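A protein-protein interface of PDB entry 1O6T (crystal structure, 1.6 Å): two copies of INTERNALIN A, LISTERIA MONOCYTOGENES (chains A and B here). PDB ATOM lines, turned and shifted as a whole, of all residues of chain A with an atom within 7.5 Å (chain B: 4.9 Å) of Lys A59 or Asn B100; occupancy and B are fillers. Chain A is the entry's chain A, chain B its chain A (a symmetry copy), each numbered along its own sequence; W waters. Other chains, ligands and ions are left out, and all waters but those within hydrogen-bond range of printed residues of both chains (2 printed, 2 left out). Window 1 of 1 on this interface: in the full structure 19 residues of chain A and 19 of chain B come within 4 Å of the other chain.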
ATOM      1  N   ASP A  20      18.825  26.804 -30.811  1.00  0.00           N
ATOM      2  CA  ASP A  20      18.580  25.372 -30.779  1.00  0.00           C
ATOM      3  C   ASP A  20      19.371  24.784 -31.983  1.00  0.00           C
ATOM      4  O   ASP A  20      19.198  25.232 -33.120  1.00  0.00           O
ATOM      5  CB  ASP A  20      17.082  25.090 -30.987  1.00  0.00           C
ATOM      6  CG  ASP A  20      16.755  23.685 -30.921  1.00  0.00           C
ATOM      7  OD1 ASP A  20      16.991  22.989 -31.949  1.00  0.00           O
ATOM      8  OD2 ASP A  20      16.282  23.140 -29.894  1.00  0.00           O
ATOM      9  N   THR A  21      20.231  23.806 -31.705  1.00  0.00           N
ATOM     10  CA  THR A  21      21.140  23.322 -32.764  1.00  0.00           C
ATOM     11  C   THR A  21      20.384  22.656 -33.897  1.00  0.00           C
ATOM     12  O   THR A  21      20.822  22.772 -35.032  1.00  0.00           O
ATOM     13  CB  THR A  21      22.192  22.407 -32.247  1.00  0.00           C
ATOM     14  OG1 THR A  21      21.626  21.313 -31.575  1.00  0.00           O
ATOM     15  CG2 THR A  21      23.129  23.113 -31.237  1.00  0.00           C
ATOM     16  N   ALA A  22      19.273  21.960 -33.592  1.00  0.00           N
ATOM     17  CA  ALA A  22      18.493  21.315 -34.626  1.00  0.00           C
ATOM     18  C   ALA A  22      17.837  22.360 -35.490  1.00  0.00           C
ATOM     19  O   ALA A  22      17.757  22.216 -36.709  1.00  0.00           O
ATOM     20  CB  ALA A  22      17.468  20.391 -34.051  1.00  0.00           C
ATOM     21  N   LEU A  23      17.319  23.414 -34.896  1.00  0.00           N
ATOM     22  CA  LEU A  23      16.740  24.451 -35.724  1.00  0.00           C
ATOM     23  C   LEU A  23      17.810  25.166 -36.577  1.00  0.00           C
ATOM     24  O   LEU A  23      17.547  25.507 -37.711  1.00  0.00           O
ATOM     25  CB  LEU A  23      15.930  25.450 -34.906  1.00  0.00           C
ATOM     26  CG  LEU A  23      15.172  26.491 -35.686  1.00  0.00           C
ATOM     27  CD1 LEU A  23      14.261  25.975 -36.756  1.00  0.00           C
ATOM     28  CD2 LEU A  23      14.360  27.380 -34.724  1.00  0.00           C
ATOM     29  N   LEU A  56      12.261  16.998 -35.762  1.00  0.00           N
ATOM     30  CA  LEU A  56      13.667  17.362 -35.799  1.00  0.00           C
ATOM     31  C   LEU A  56      14.309  17.469 -34.412  1.00  0.00           C
ATOM     32  O   LEU A  56      15.491  17.819 -34.332  1.00  0.00           O
ATOM     33  CB  LEU A  56      13.833  18.666 -36.544  1.00  0.00           C
ATOM     34  CG  LEU A  56      13.609  18.608 -38.059  1.00  0.00           C
ATOM     35  CD1 LEU A  56      13.720  19.972 -38.601  1.00  0.00           C
ATOM     36  CD2 LEU A  56      14.587  17.642 -38.752  1.00  0.00           C
ATOM     37  N   GLY A  57      13.590  17.176 -33.363  1.00  0.00           N
ATOM     38  CA  GLY A  57      14.139  17.288 -32.025  1.00  0.00           C
ATOM     39  C   GLY A  57      14.391  18.722 -31.644  1.00  0.00           C
ATOM     40  O   GLY A  57      15.309  19.029 -30.889  1.00  0.00           O
ATOM     41  N   ILE A  58      13.565  19.625 -32.150  1.00  0.00           N
ATOM     42  CA  ILE A  58      13.684  21.050 -31.772  1.00  0.00           C
ATOM     43  C   ILE A  58      13.047  21.338 -30.386  1.00  0.00           C
ATOM     44  O   ILE A  58      11.870  21.005 -30.124  1.00  0.00           O
ATOM     45  CB  ILE A  58      13.048  21.931 -32.870  1.00  0.00           C
ATOM     46  CG1 ILE A  58      13.864  21.795 -34.175  1.00  0.00           C
ATOM     47  CG2 ILE A  58      13.062  23.375 -32.437  1.00  0.00           C
ATOM     48  CD1 ILE A  58      13.164  22.256 -35.316  1.00  0.00           C
ATOM     49  N   LYS A  59      13.825  21.956 -29.517  1.00  0.00           N
ATOM     50  CA  LYS A  59      13.341  22.296 -28.158  1.00  0.00           C
ATOM     51  C   LYS A  59      13.046  23.753 -27.978  1.00  0.00           C
ATOM     52  O   LYS A  59      12.328  24.114 -27.034  1.00  0.00           O
ATOM     53  CB  LYS A  59      14.368  21.816 -27.094  1.00  0.00           C
ATOM     54  CG  LYS A  59      14.571  20.273 -27.171  1.00  0.00           C
ATOM     55  CD  LYS A  59      15.985  19.851 -27.362  1.00  0.00           C
ATOM     56  CE  LYS A  59      16.180  18.397 -27.292  1.00  0.00           C
ATOM     57  NZ  LYS A  59      15.541  17.636 -28.451  1.00  0.00           N
ATOM     58  N   SER A  60      13.554  24.601 -28.844  1.00  0.00           N
ATOM     59  CA  SER A  60      13.343  26.038 -28.760  1.00  0.00           C
ATOM     60  C   SER A  60      13.247  26.595 -30.147  1.00  0.00           C
ATOM     61  O   SER A  60      14.045  26.189 -31.046  1.00  0.00           O
ATOM     62  CB  SER A  60      14.535  26.716 -28.075  1.00  0.00           C
ATOM     63  OG  SER A  60      14.416  28.112 -28.160  1.00  0.00           O
ATOM     64  N   ILE A  61      12.318  27.518 -30.359  1.00  0.00           N
ATOM     65  CA  ILE A  61      12.214  28.203 -31.613  1.00  0.00           C
ATOM     66  C   ILE A  61      12.740  29.624 -31.542  1.00  0.00           C
ATOM     67  O   ILE A  61      12.409  30.425 -32.401  1.00  0.00           O
ATOM     68  CB  ILE A  61      10.828  28.177 -32.198  1.00  0.00           C
ATOM     69  CG1 ILE A  61       9.751  28.591 -31.197  1.00  0.00           C
ATOM     70  CG2 ILE A  61      10.515  26.759 -32.690  1.00  0.00           C
ATOM     71  CD1 ILE A  61       8.412  28.895 -31.810  1.00  0.00           C
ATOM     72  N   ASP A  62      13.596  29.899 -30.554  1.00  0.00           N
ATOM     73  CA  ASP A  62      14.307  31.176 -30.546  1.00  0.00           C
ATOM     74  C   ASP A  62      14.966  31.426 -31.858  1.00  0.00           C
ATOM     75  O   ASP A  62      15.635  30.539 -32.413  1.00  0.00           O
ATOM     76  CB  ASP A  62      15.361  31.200 -29.431  1.00  0.00           C
ATOM     77  CG  ASP A  62      14.729  31.342 -28.042  1.00  0.00           C
ATOM     78  OD1 ASP A  62      13.452  31.406 -27.920  1.00  0.00           O
ATOM     79  OD2 ASP A  62      15.433  31.379 -27.008  1.00  0.00           O
ATOM     80  N   ASN A  78       7.965  17.716 -32.018  1.00  0.00           N
ATOM     81  CA  ASN A  78       9.206  18.267 -31.442  1.00  0.00           C
ATOM     82  C   ASN A  78       9.065  18.358 -29.936  1.00  0.00           C
ATOM     83  O   ASN A  78       8.224  17.654 -29.356  1.00  0.00           O
ATOM     84  CB  ASN A  78       9.510  19.626 -32.089  1.00  0.00           C
ATOM     85  CG  ASN A  78      10.104  19.515 -33.491  1.00  0.00           C
ATOM     86  OD1 ASN A  78      11.158  18.892 -33.661  1.00  0.00           O
ATOM     87  ND2 ASN A  78       9.450  20.158 -34.518  1.00  0.00           N
ATOM     88  N   GLN A  79       9.891  19.146 -29.270  1.00  0.00           N
ATOM     89  CA  GLN A  79       9.783  19.271 -27.807  1.00  0.00           C
ATOM     90  C   GLN A  79       9.514  20.701 -27.416  1.00  0.00           C
ATOM     91  O   GLN A  79      10.050  21.193 -26.426  1.00  0.00           O
ATOM     92  CB  GLN A  79      11.014  18.723 -27.093  1.00  0.00           C
ATOM     93  CG  GLN A  79      11.267  17.196 -27.395  1.00  0.00           C
ATOM     94  CD  GLN A  79      11.819  16.937 -28.762  1.00  0.00           C
ATOM     95  OE1 GLN A  79      12.812  17.559 -29.165  1.00  0.00           O
ATOM     96  NE2 GLN A  79      11.153  16.014 -29.549  1.00  0.00           N
ATOM     97  N   LEU A  80       8.711  21.385 -28.184  1.00  0.00           N
ATOM     98  CA  LEU A  80       8.436  22.790 -27.874  1.00  0.00           C
ATOM     99  C   LEU A  80       7.632  22.943 -26.647  1.00  0.00           C
ATOM    100  O   LEU A  80       6.685  22.189 -26.370  1.00  0.00           O
ATOM    101  CB  LEU A  80       7.736  23.494 -29.009  1.00  0.00           C
ATOM    102  CG  LEU A  80       8.397  23.513 -30.380  1.00  0.00           C
ATOM    103  CD1 LEU A  80       7.612  24.337 -31.316  1.00  0.00           C
ATOM    104  CD2 LEU A  80       9.846  23.970 -30.261  1.00  0.00           C
ATOM    105  N   THR A  81       8.042  23.903 -25.823  1.00  0.00           N
ATOM    106  CA  THR A  81       7.300  24.254 -24.628  1.00  0.00           C
ATOM    107  C   THR A  81       6.913  25.720 -24.781  1.00  0.00           C
ATOM    108  O   THR A  81       5.746  26.058 -24.900  1.00  0.00           O
ATOM    109  CB  THR A  81       8.093  23.971 -23.331  1.00  0.00           C
ATOM    110  OG1 THR A  81       9.444  24.497 -23.389  1.00  0.00           O
ATOM    111  CG2 THR A  81       8.275  22.470 -23.128  1.00  0.00           C
ATOM    112  N   ASP A  82       7.920  26.570 -24.856  1.00  0.00           N
ATOM    113  CA  ASP A  82       7.769  28.024 -24.951  1.00  0.00           C
ATOM    114  C   ASP A  82       7.700  28.480 -26.409  1.00  0.00           C
ATOM    115  O   ASP A  82       8.689  28.277 -27.184  1.00  0.00           O
ATOM    116  CB  ASP A  82       8.976  28.662 -24.272  1.00  0.00           C
ATOM    117  CG  ASP A  82       9.023  30.159 -24.406  1.00  0.00           C
ATOM    118  OD1 ASP A  82       7.950  30.781 -24.461  1.00  0.00           O
ATOM    119  OD2 ASP A  82      10.137  30.801 -24.425  1.00  0.00           O
ATOM    120  N   ASN A 100       3.748  18.335 -29.205  1.00  0.00           N
ATOM    121  CA  ASN A 100       4.808  19.071 -28.516  1.00  0.00           C
ATOM    122  C   ASN A 100       4.426  19.012 -27.048  1.00  0.00           C
ATOM    123  O   ASN A 100       3.626  18.148 -26.637  1.00  0.00           O
ATOM    124  CB  ASN A 100       4.968  20.478 -29.077  1.00  0.00           C
ATOM    125  CG  ASN A 100       5.758  20.466 -30.362  1.00  0.00           C
ATOM    126  OD1 ASN A 100       6.973  20.313 -30.342  1.00  0.00           O
ATOM    127  ND2 ASN A 100       5.076  20.606 -31.493  1.00  0.00           N
ATOM    128  N   PHE B  75      11.103   5.086 -28.587  1.00  0.00           N
ATOM    129  CA  PHE B  75      10.293   6.208 -28.165  1.00  0.00           C
ATOM    130  C   PHE B  75      10.859   7.526 -28.740  1.00  0.00           C
ATOM    131  O   PHE B  75      10.662   8.618 -28.204  1.00  0.00           O
ATOM    132  CB  PHE B  75      10.175   6.335 -26.616  1.00  0.00           C
ATOM    133  CG  PHE B  75       9.247   5.353 -26.013  1.00  0.00           C
ATOM    134  CD1 PHE B  75       7.896   5.613 -25.993  1.00  0.00           C
ATOM    135  CD2 PHE B  75       9.685   4.205 -25.475  1.00  0.00           C
ATOM    136  CE1 PHE B  75       6.997   4.691 -25.444  1.00  0.00           C
ATOM    137  CE2 PHE B  75       8.778   3.282 -24.926  1.00  0.00           C
ATOM    138  CZ  PHE B  75       7.455   3.563 -24.926  1.00  0.00           C
ATOM    139  N   SER B  76      11.553   7.427 -29.857  1.00  0.00           N
ATOM    140  CA  SER B  76      12.101   8.607 -30.495  1.00  0.00           C
ATOM    141  C   SER B  76      11.014   9.601 -30.898  1.00  0.00           C
ATOM    142  O   SER B  76       9.856   9.230 -31.167  1.00  0.00           O
ATOM    143  CB  SER B  76      12.998   8.180 -31.620  1.00  0.00           C
ATOM    144  OG  SER B  76      12.274   7.724 -32.685  1.00  0.00           O
ATOM    145  N   ASN B  77      11.371  10.908 -30.951  1.00  0.00           N
ATOM    146  CA  ASN B  77      10.473  11.921 -31.450  1.00  0.00           C
ATOM    147  C   ASN B  77       9.206  11.997 -30.659  1.00  0.00           C
ATOM    148  O   ASN B  77       8.112  11.949 -31.166  1.00  0.00           O
ATOM    149  CB  ASN B  77      10.157  11.711 -32.955  1.00  0.00           C
ATOM    150  CG  ASN B  77      11.316  12.044 -33.828  1.00  0.00           C
ATOM    151  OD1 ASN B  77      11.851  13.098 -33.783  1.00  0.00           O
ATOM    152  ND2 ASN B  77      11.713  11.080 -34.660  1.00  0.00           N
ATOM    153  N   ASN B  78       9.389  12.142 -29.351  1.00  0.00           N
ATOM    154  CA  ASN B  78       8.292  12.364 -28.389  1.00  0.00           C
ATOM    155  C   ASN B  78       8.664  13.499 -27.456  1.00  0.00           C
ATOM    156  O   ASN B  78       9.527  14.320 -27.804  1.00  0.00           O
ATOM    157  CB  ASN B  78       7.999  11.057 -27.639  1.00  0.00           C
ATOM    158  CG  ASN B  78       7.195  10.051 -28.459  1.00  0.00           C
ATOM    159  OD1 ASN B  78       6.083  10.368 -28.898  1.00  0.00           O
ATOM    160  ND2 ASN B  78       7.734   8.798 -28.646  1.00  0.00           N
ATOM    161  N   GLN B  79       8.008  13.619 -26.314  1.00  0.00           N
ATOM    162  CA  GLN B  79       8.343  14.701 -25.375  1.00  0.00           C
ATOM    163  C   GLN B  79       8.775  14.136 -24.046  1.00  0.00           C
ATOM    164  O   GLN B  79       8.431  14.669 -22.995  1.00  0.00           O
ATOM    165  CB  GLN B  79       7.195  15.691 -25.209  1.00  0.00           C
ATOM    166  CG  GLN B  79       6.786  16.386 -26.565  1.00  0.00           C
ATOM    167  CD  GLN B  79       6.018  15.493 -27.489  1.00  0.00           C
ATOM    168  OE1 GLN B  79       5.025  14.874 -27.081  1.00  0.00           O
ATOM    169  NE2 GLN B  79       6.487  15.370 -28.785  1.00  0.00           N
ATOM    170  N   LEU B  80       9.503  13.053 -24.071  1.00  0.00           N
ATOM    171  CA  LEU B  80       9.926  12.437 -22.811  1.00  0.00           C
ATOM    172  C   LEU B  80      10.913  13.263 -22.092  1.00  0.00           C
ATOM    173  O   LEU B  80      11.832  13.865 -22.672  1.00  0.00           O
ATOM    174  CB  LEU B  80      10.499  11.059 -23.019  1.00  0.00           C
ATOM    175  CG  LEU B  80       9.644  10.004 -23.708  1.00  0.00           C
ATOM    176  CD1 LEU B  80      10.339   8.705 -23.717  1.00  0.00           C
ATOM    177  CD2 LEU B  80       8.267   9.934 -23.058  1.00  0.00           C
ATOM    178  N   MET B  97      15.750   6.507 -28.316  1.00  0.00           N
ATOM    179  CA  MET B  97      15.055   7.601 -27.645  1.00  0.00           C
ATOM    180  C   MET B  97      15.685   8.928 -27.998  1.00  0.00           C
ATOM    181  O   MET B  97      15.682   9.843 -27.216  1.00  0.00           O
ATOM    182  CB  MET B  97      15.000   7.427 -26.120  1.00  0.00           C
ATOM    183  CG  MET B  97      14.067   6.386 -25.652  1.00  0.00           C
ATOM    184  SD  MET B  97      13.640   6.725 -23.885  1.00  0.00           S
ATOM    185  CE  MET B  97      15.330   6.613 -23.091  1.00  0.00           C
ATOM    186  N   ASN B  98      16.207   9.010 -29.211  1.00  0.00           N
ATOM    187  CA  ASN B  98      16.620  10.301 -29.756  1.00  0.00           C
ATOM    188  C   ASN B  98      15.435  11.254 -29.894  1.00  0.00           C
ATOM    189  O   ASN B  98      14.260  10.831 -29.971  1.00  0.00           O
ATOM    190  CB  ASN B  98      17.288  10.154 -31.091  1.00  0.00           C
ATOM    191  CG  ASN B  98      16.453   9.497 -32.070  1.00  0.00           C
ATOM    192  OD1 ASN B  98      15.985  10.143 -33.057  1.00  0.00           O
ATOM    193  ND2 ASN B  98      16.227   8.212 -31.868  1.00  0.00           N
ATOM    194  N   ASN B  99      15.720  12.549 -29.936  1.00  0.00           N
ATOM    195  CA  ASN B  99      14.690  13.571 -30.152  1.00  0.00           C
ATOM    196  C   ASN B  99      13.586  13.489 -29.110  1.00  0.00           C
ATOM    197  O   ASN B  99      12.404  13.254 -29.388  1.00  0.00           O
ATOM    198  CB  ASN B  99      14.101  13.461 -31.559  1.00  0.00           C
ATOM    199  CG  ASN B  99      15.112  13.687 -32.652  1.00  0.00           C
ATOM    200  OD1 ASN B  99      16.294  13.893 -32.394  1.00  0.00           O
ATOM    201  ND2 ASN B  99      14.647  13.717 -33.906  1.00  0.00           N
ATOM    202  N   ASN B 100      14.013  13.695 -27.841  1.00  0.00           N
ATOM    203  CA  ASN B 100      13.126  13.883 -26.694  1.00  0.00           C
ATOM    204  C   ASN B 100      13.719  15.059 -25.938  1.00  0.00           C
ATOM    205  O   ASN B 100      14.504  15.845 -26.506  1.00  0.00           O
ATOM    206  CB  ASN B 100      12.991  12.604 -25.877  1.00  0.00           C
ATOM    207  CG  ASN B 100      12.019  11.647 -26.520  1.00  0.00           C
ATOM    208  OD1 ASN B 100      10.812  11.846 -26.449  1.00  0.00           O
ATOM    209  ND2 ASN B 100      12.533  10.610 -27.173  1.00  0.00           N
ATOM    210  N   GLN B 101      13.310  15.246 -24.674  1.00  0.00           N
ATOM    211  CA  GLN B 101      13.910  16.259 -23.860  1.00  0.00           C
ATOM    212  C   GLN B 101      14.385  15.654 -22.544  1.00  0.00           C
ATOM    213  O   GLN B 101      14.119  16.187 -21.448  1.00  0.00           O
ATOM    214  CB  GLN B 101      12.978  17.457 -23.631  1.00  0.00           C
ATOM    215  CG  GLN B 101      13.745  18.652 -22.989  1.00  0.00           C
ATOM    216  CD  GLN B 101      12.985  19.985 -22.909  1.00  0.00           C
ATOM    217  OE1 GLN B 101      12.514  20.514 -23.911  1.00  0.00           O
ATOM    218  NE2 GLN B 101      12.901  20.548 -21.679  1.00  0.00           N
ATOM    219  N   ILE B 102      15.078  14.536 -22.638  1.00  0.00           N
ATOM    220  CA  ILE B 102      15.593  13.844 -21.474  1.00  0.00           C
ATOM    221  C   ILE B 102      16.813  14.520 -20.978  1.00  0.00           C
ATOM    222  O   ILE B 102      17.697  14.861 -21.745  1.00  0.00           O
ATOM    223  CB  ILE B 102      15.916  12.403 -21.867  1.00  0.00           C
ATOM    224  CG1 ILE B 102      14.611  11.678 -22.279  1.00  0.00           C
ATOM    225  CG2 ILE B 102      16.520  11.652 -20.750  1.00  0.00           C
ATOM    226  CD1 ILE B 102      14.873  10.488 -23.137  1.00  0.00           C
ATOM    227  N   ASN B 121      20.217  14.288 -29.469  1.00  0.00           N
ATOM    228  CA  ASN B 121      19.286  15.411 -29.433  1.00  0.00           C
ATOM    229  C   ASN B 121      18.287  15.312 -28.282  1.00  0.00           C
ATOM    230  O   ASN B 121      17.066  15.236 -28.472  1.00  0.00           O
ATOM    231  CB  ASN B 121      18.594  15.607 -30.776  1.00  0.00           C
ATOM    232  CG  ASN B 121      18.051  16.952 -30.926  1.00  0.00           C
ATOM    233  OD1 ASN B 121      18.088  17.793 -29.966  1.00  0.00           O
ATOM    234  ND2 ASN B 121      17.516  17.243 -32.154  1.00  0.00           N
ATOM    235  N   ASN B 122      18.844  15.264 -27.066  1.00  0.00           N
ATOM    236  CA  ASN B 122      18.086  15.362 -25.836  1.00  0.00           C
ATOM    237  C   ASN B 122      18.701  16.564 -25.084  1.00  0.00           C
ATOM    238  O   ASN B 122      19.315  17.469 -25.720  1.00  0.00           O
ATOM    239  CB  ASN B 122      18.158  14.029 -25.103  1.00  0.00           C
ATOM    240  CG  ASN B 122      17.051  13.110 -25.549  1.00  0.00           C
ATOM    241  OD1 ASN B 122      15.908  13.342 -25.202  1.00  0.00           O
ATOM    242  ND2 ASN B 122      17.380  12.070 -26.351  1.00  0.00           N
ATOM    243  N   GLN B 123      18.597  16.558 -23.765  1.00  0.00           N
ATOM    244  CA  GLN B 123      19.162  17.635 -22.953  1.00  0.00           C
ATOM    245  C   GLN B 123      20.038  17.053 -21.877  1.00  0.00           C
ATOM    246  O   GLN B 123      20.030  17.471 -20.714  1.00  0.00           O
ATOM    247  CB  GLN B 123      18.076  18.553 -22.390  1.00  0.00           C
ATOM    248  CG  GLN B 123      17.438  19.414 -23.451  1.00  0.00           C
ATOM    249  CD  GLN B 123      16.528  20.472 -22.850  1.00  0.00           C
ATOM    250  OE1 GLN B 123      16.177  20.405 -21.624  1.00  0.00           O
ATOM    251  NE2 GLN B 123      16.149  21.446 -23.657  1.00  0.00           N
HETATM  252  O   HOH W   1      20.466  20.037 -29.163  1.00  0.00           O
HETATM  253  O   HOH W   2      11.364  15.493 -32.482  1.00  0.00           O
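NZ of Lys A59 lies within hydrogen-bond range of O of Asn B121, at 2.8 Å. NE2 of Gln A79 sits at hydrogen-bond distance from O of Asn B78 (2.9 Å). The side-chain amide nitrogen of Gln B79 is in hydrogen-bond range of the backbone carbonyl oxygen of Asn A78 (2.9 Å). The side-chain amino group (NZ) of Lys A59 lies within hydrogen-bond range of the backbone carbonyl oxygen (O) of Asn B100, 2.8 Å away. NE2 of Gln A79 is in hydrogen-bond range of O of Asn B99 (3.0 Å). ND2 of Asn B121 sits at hydrogen-bond distance from O of Leu A56 (3.0 Å). O of Gly A57 sits at hydrogen-bond distance from ND2 of Asn B121, at 3.1 Å.
The side-chain amide oxygen (OE1) of Gln B123 lies within hydrogen-bond range of the side-chain amide nitrogen (NE2) of Gln B101 (3.3 Å). OD1 of Asn B122 sits at hydrogen-bond distance from N of Ile B102 (2.9 Å). N of Gln B101 lies within hydrogen-bond range of O of Leu B80 (2.8 Å). The backbone NH (N) of Gln A79 lies within hydrogen-bond range of the side-chain amide oxygen (OD1) of Asn A100 (3.3 Å). The backbone carbonyl oxygen of Ile B102 sits at hydrogen-bond distance from the backbone NH of Gln B123. The side-chain amide oxygen (OD1) of Asn B122 is in hydrogen-bond range of the backbone NH (N) of Gln B101, 3.3 Å away.
Ala A22 touches Asn B121 (CB to ND2, 3.7 Å). Leu A56 touches Asn B99 (C to ND2, 3.8 Å). Asn B99 touches Gly A57. CG of Lys A59 touches OE1 of Gln B101, at 3.9 Å. CE of Lys A59 touches O of Asn B122, at 3.6 Å. Lys A59 touches Gln B123. O of Asn A78 touches O of Asn B78 (3.9 Å). Gln A79 touches Asn B100. OE1 of Gln B101 touches O of Gln A79, 3.6 Å away. C of Asn A100 touches CG of Gln B79, 3.6 Å away.
Of the printed residues of chain A, Gln B79 touches Asn A78 (2.9 Å) and Asn A100 (3.6 Å). Of the printed residues of chain B, Gly A57 touches Asn B99 (3.7 Å) and Asn B121 (3.1 Å). Ser B76 touches none of the printed residues of chain A. The nearest printed residue of chain B that does not touch Lys A59 is Asn B99 (4.5 Å). The nearest residue of chain A that does not touch Asn B100 is Gly A57 (5.5 Å). The nearest printed residue of chain B that does not touch Asn A100 is Asn B78 (6.7 Å).
Along chain B the printed residues that touch a printed residue of chain A span positions 78 to 123. Printed residues of chain A that touch a printed residue of chain B: Ala A22, Leu A56, Gly A57, Lys A59, Asn A78, Gln A79 and Asn A100. Hydrophobic or aromatic side chains of chain A that line the printed part of chain B: Ala A22.
Asn A78 touches its own counterpart, Asn B78. Asn A78 touches Gln B79, and with the chains exchanged Gln A79 touches Asn B78. Gln A79 touches Asn B100, and with the chains exchanged Asn A100 touches Gln B79. Positions printed for both chains: 78, 79, 80 and 100. Of the 17 pairs that touch across the chains among the printed residues, 5 have their exchanged pair printed and touching as well.
Water W2 lies within hydrogen-bond range of the side-chain amide oxygen of Asn B77 (2.8 Å), the backbone NH of Gly A57 (2.9 Å) and the side-chain amide nitrogen of Gln A79 (3.0 Å). Water W1 lies within hydrogen-bond range of the side-chain hydroxyl (OG1) of Thr A21 (3.0 Å) and the side-chain amide oxygen (OD1) of Asn B121 (3.4 Å).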
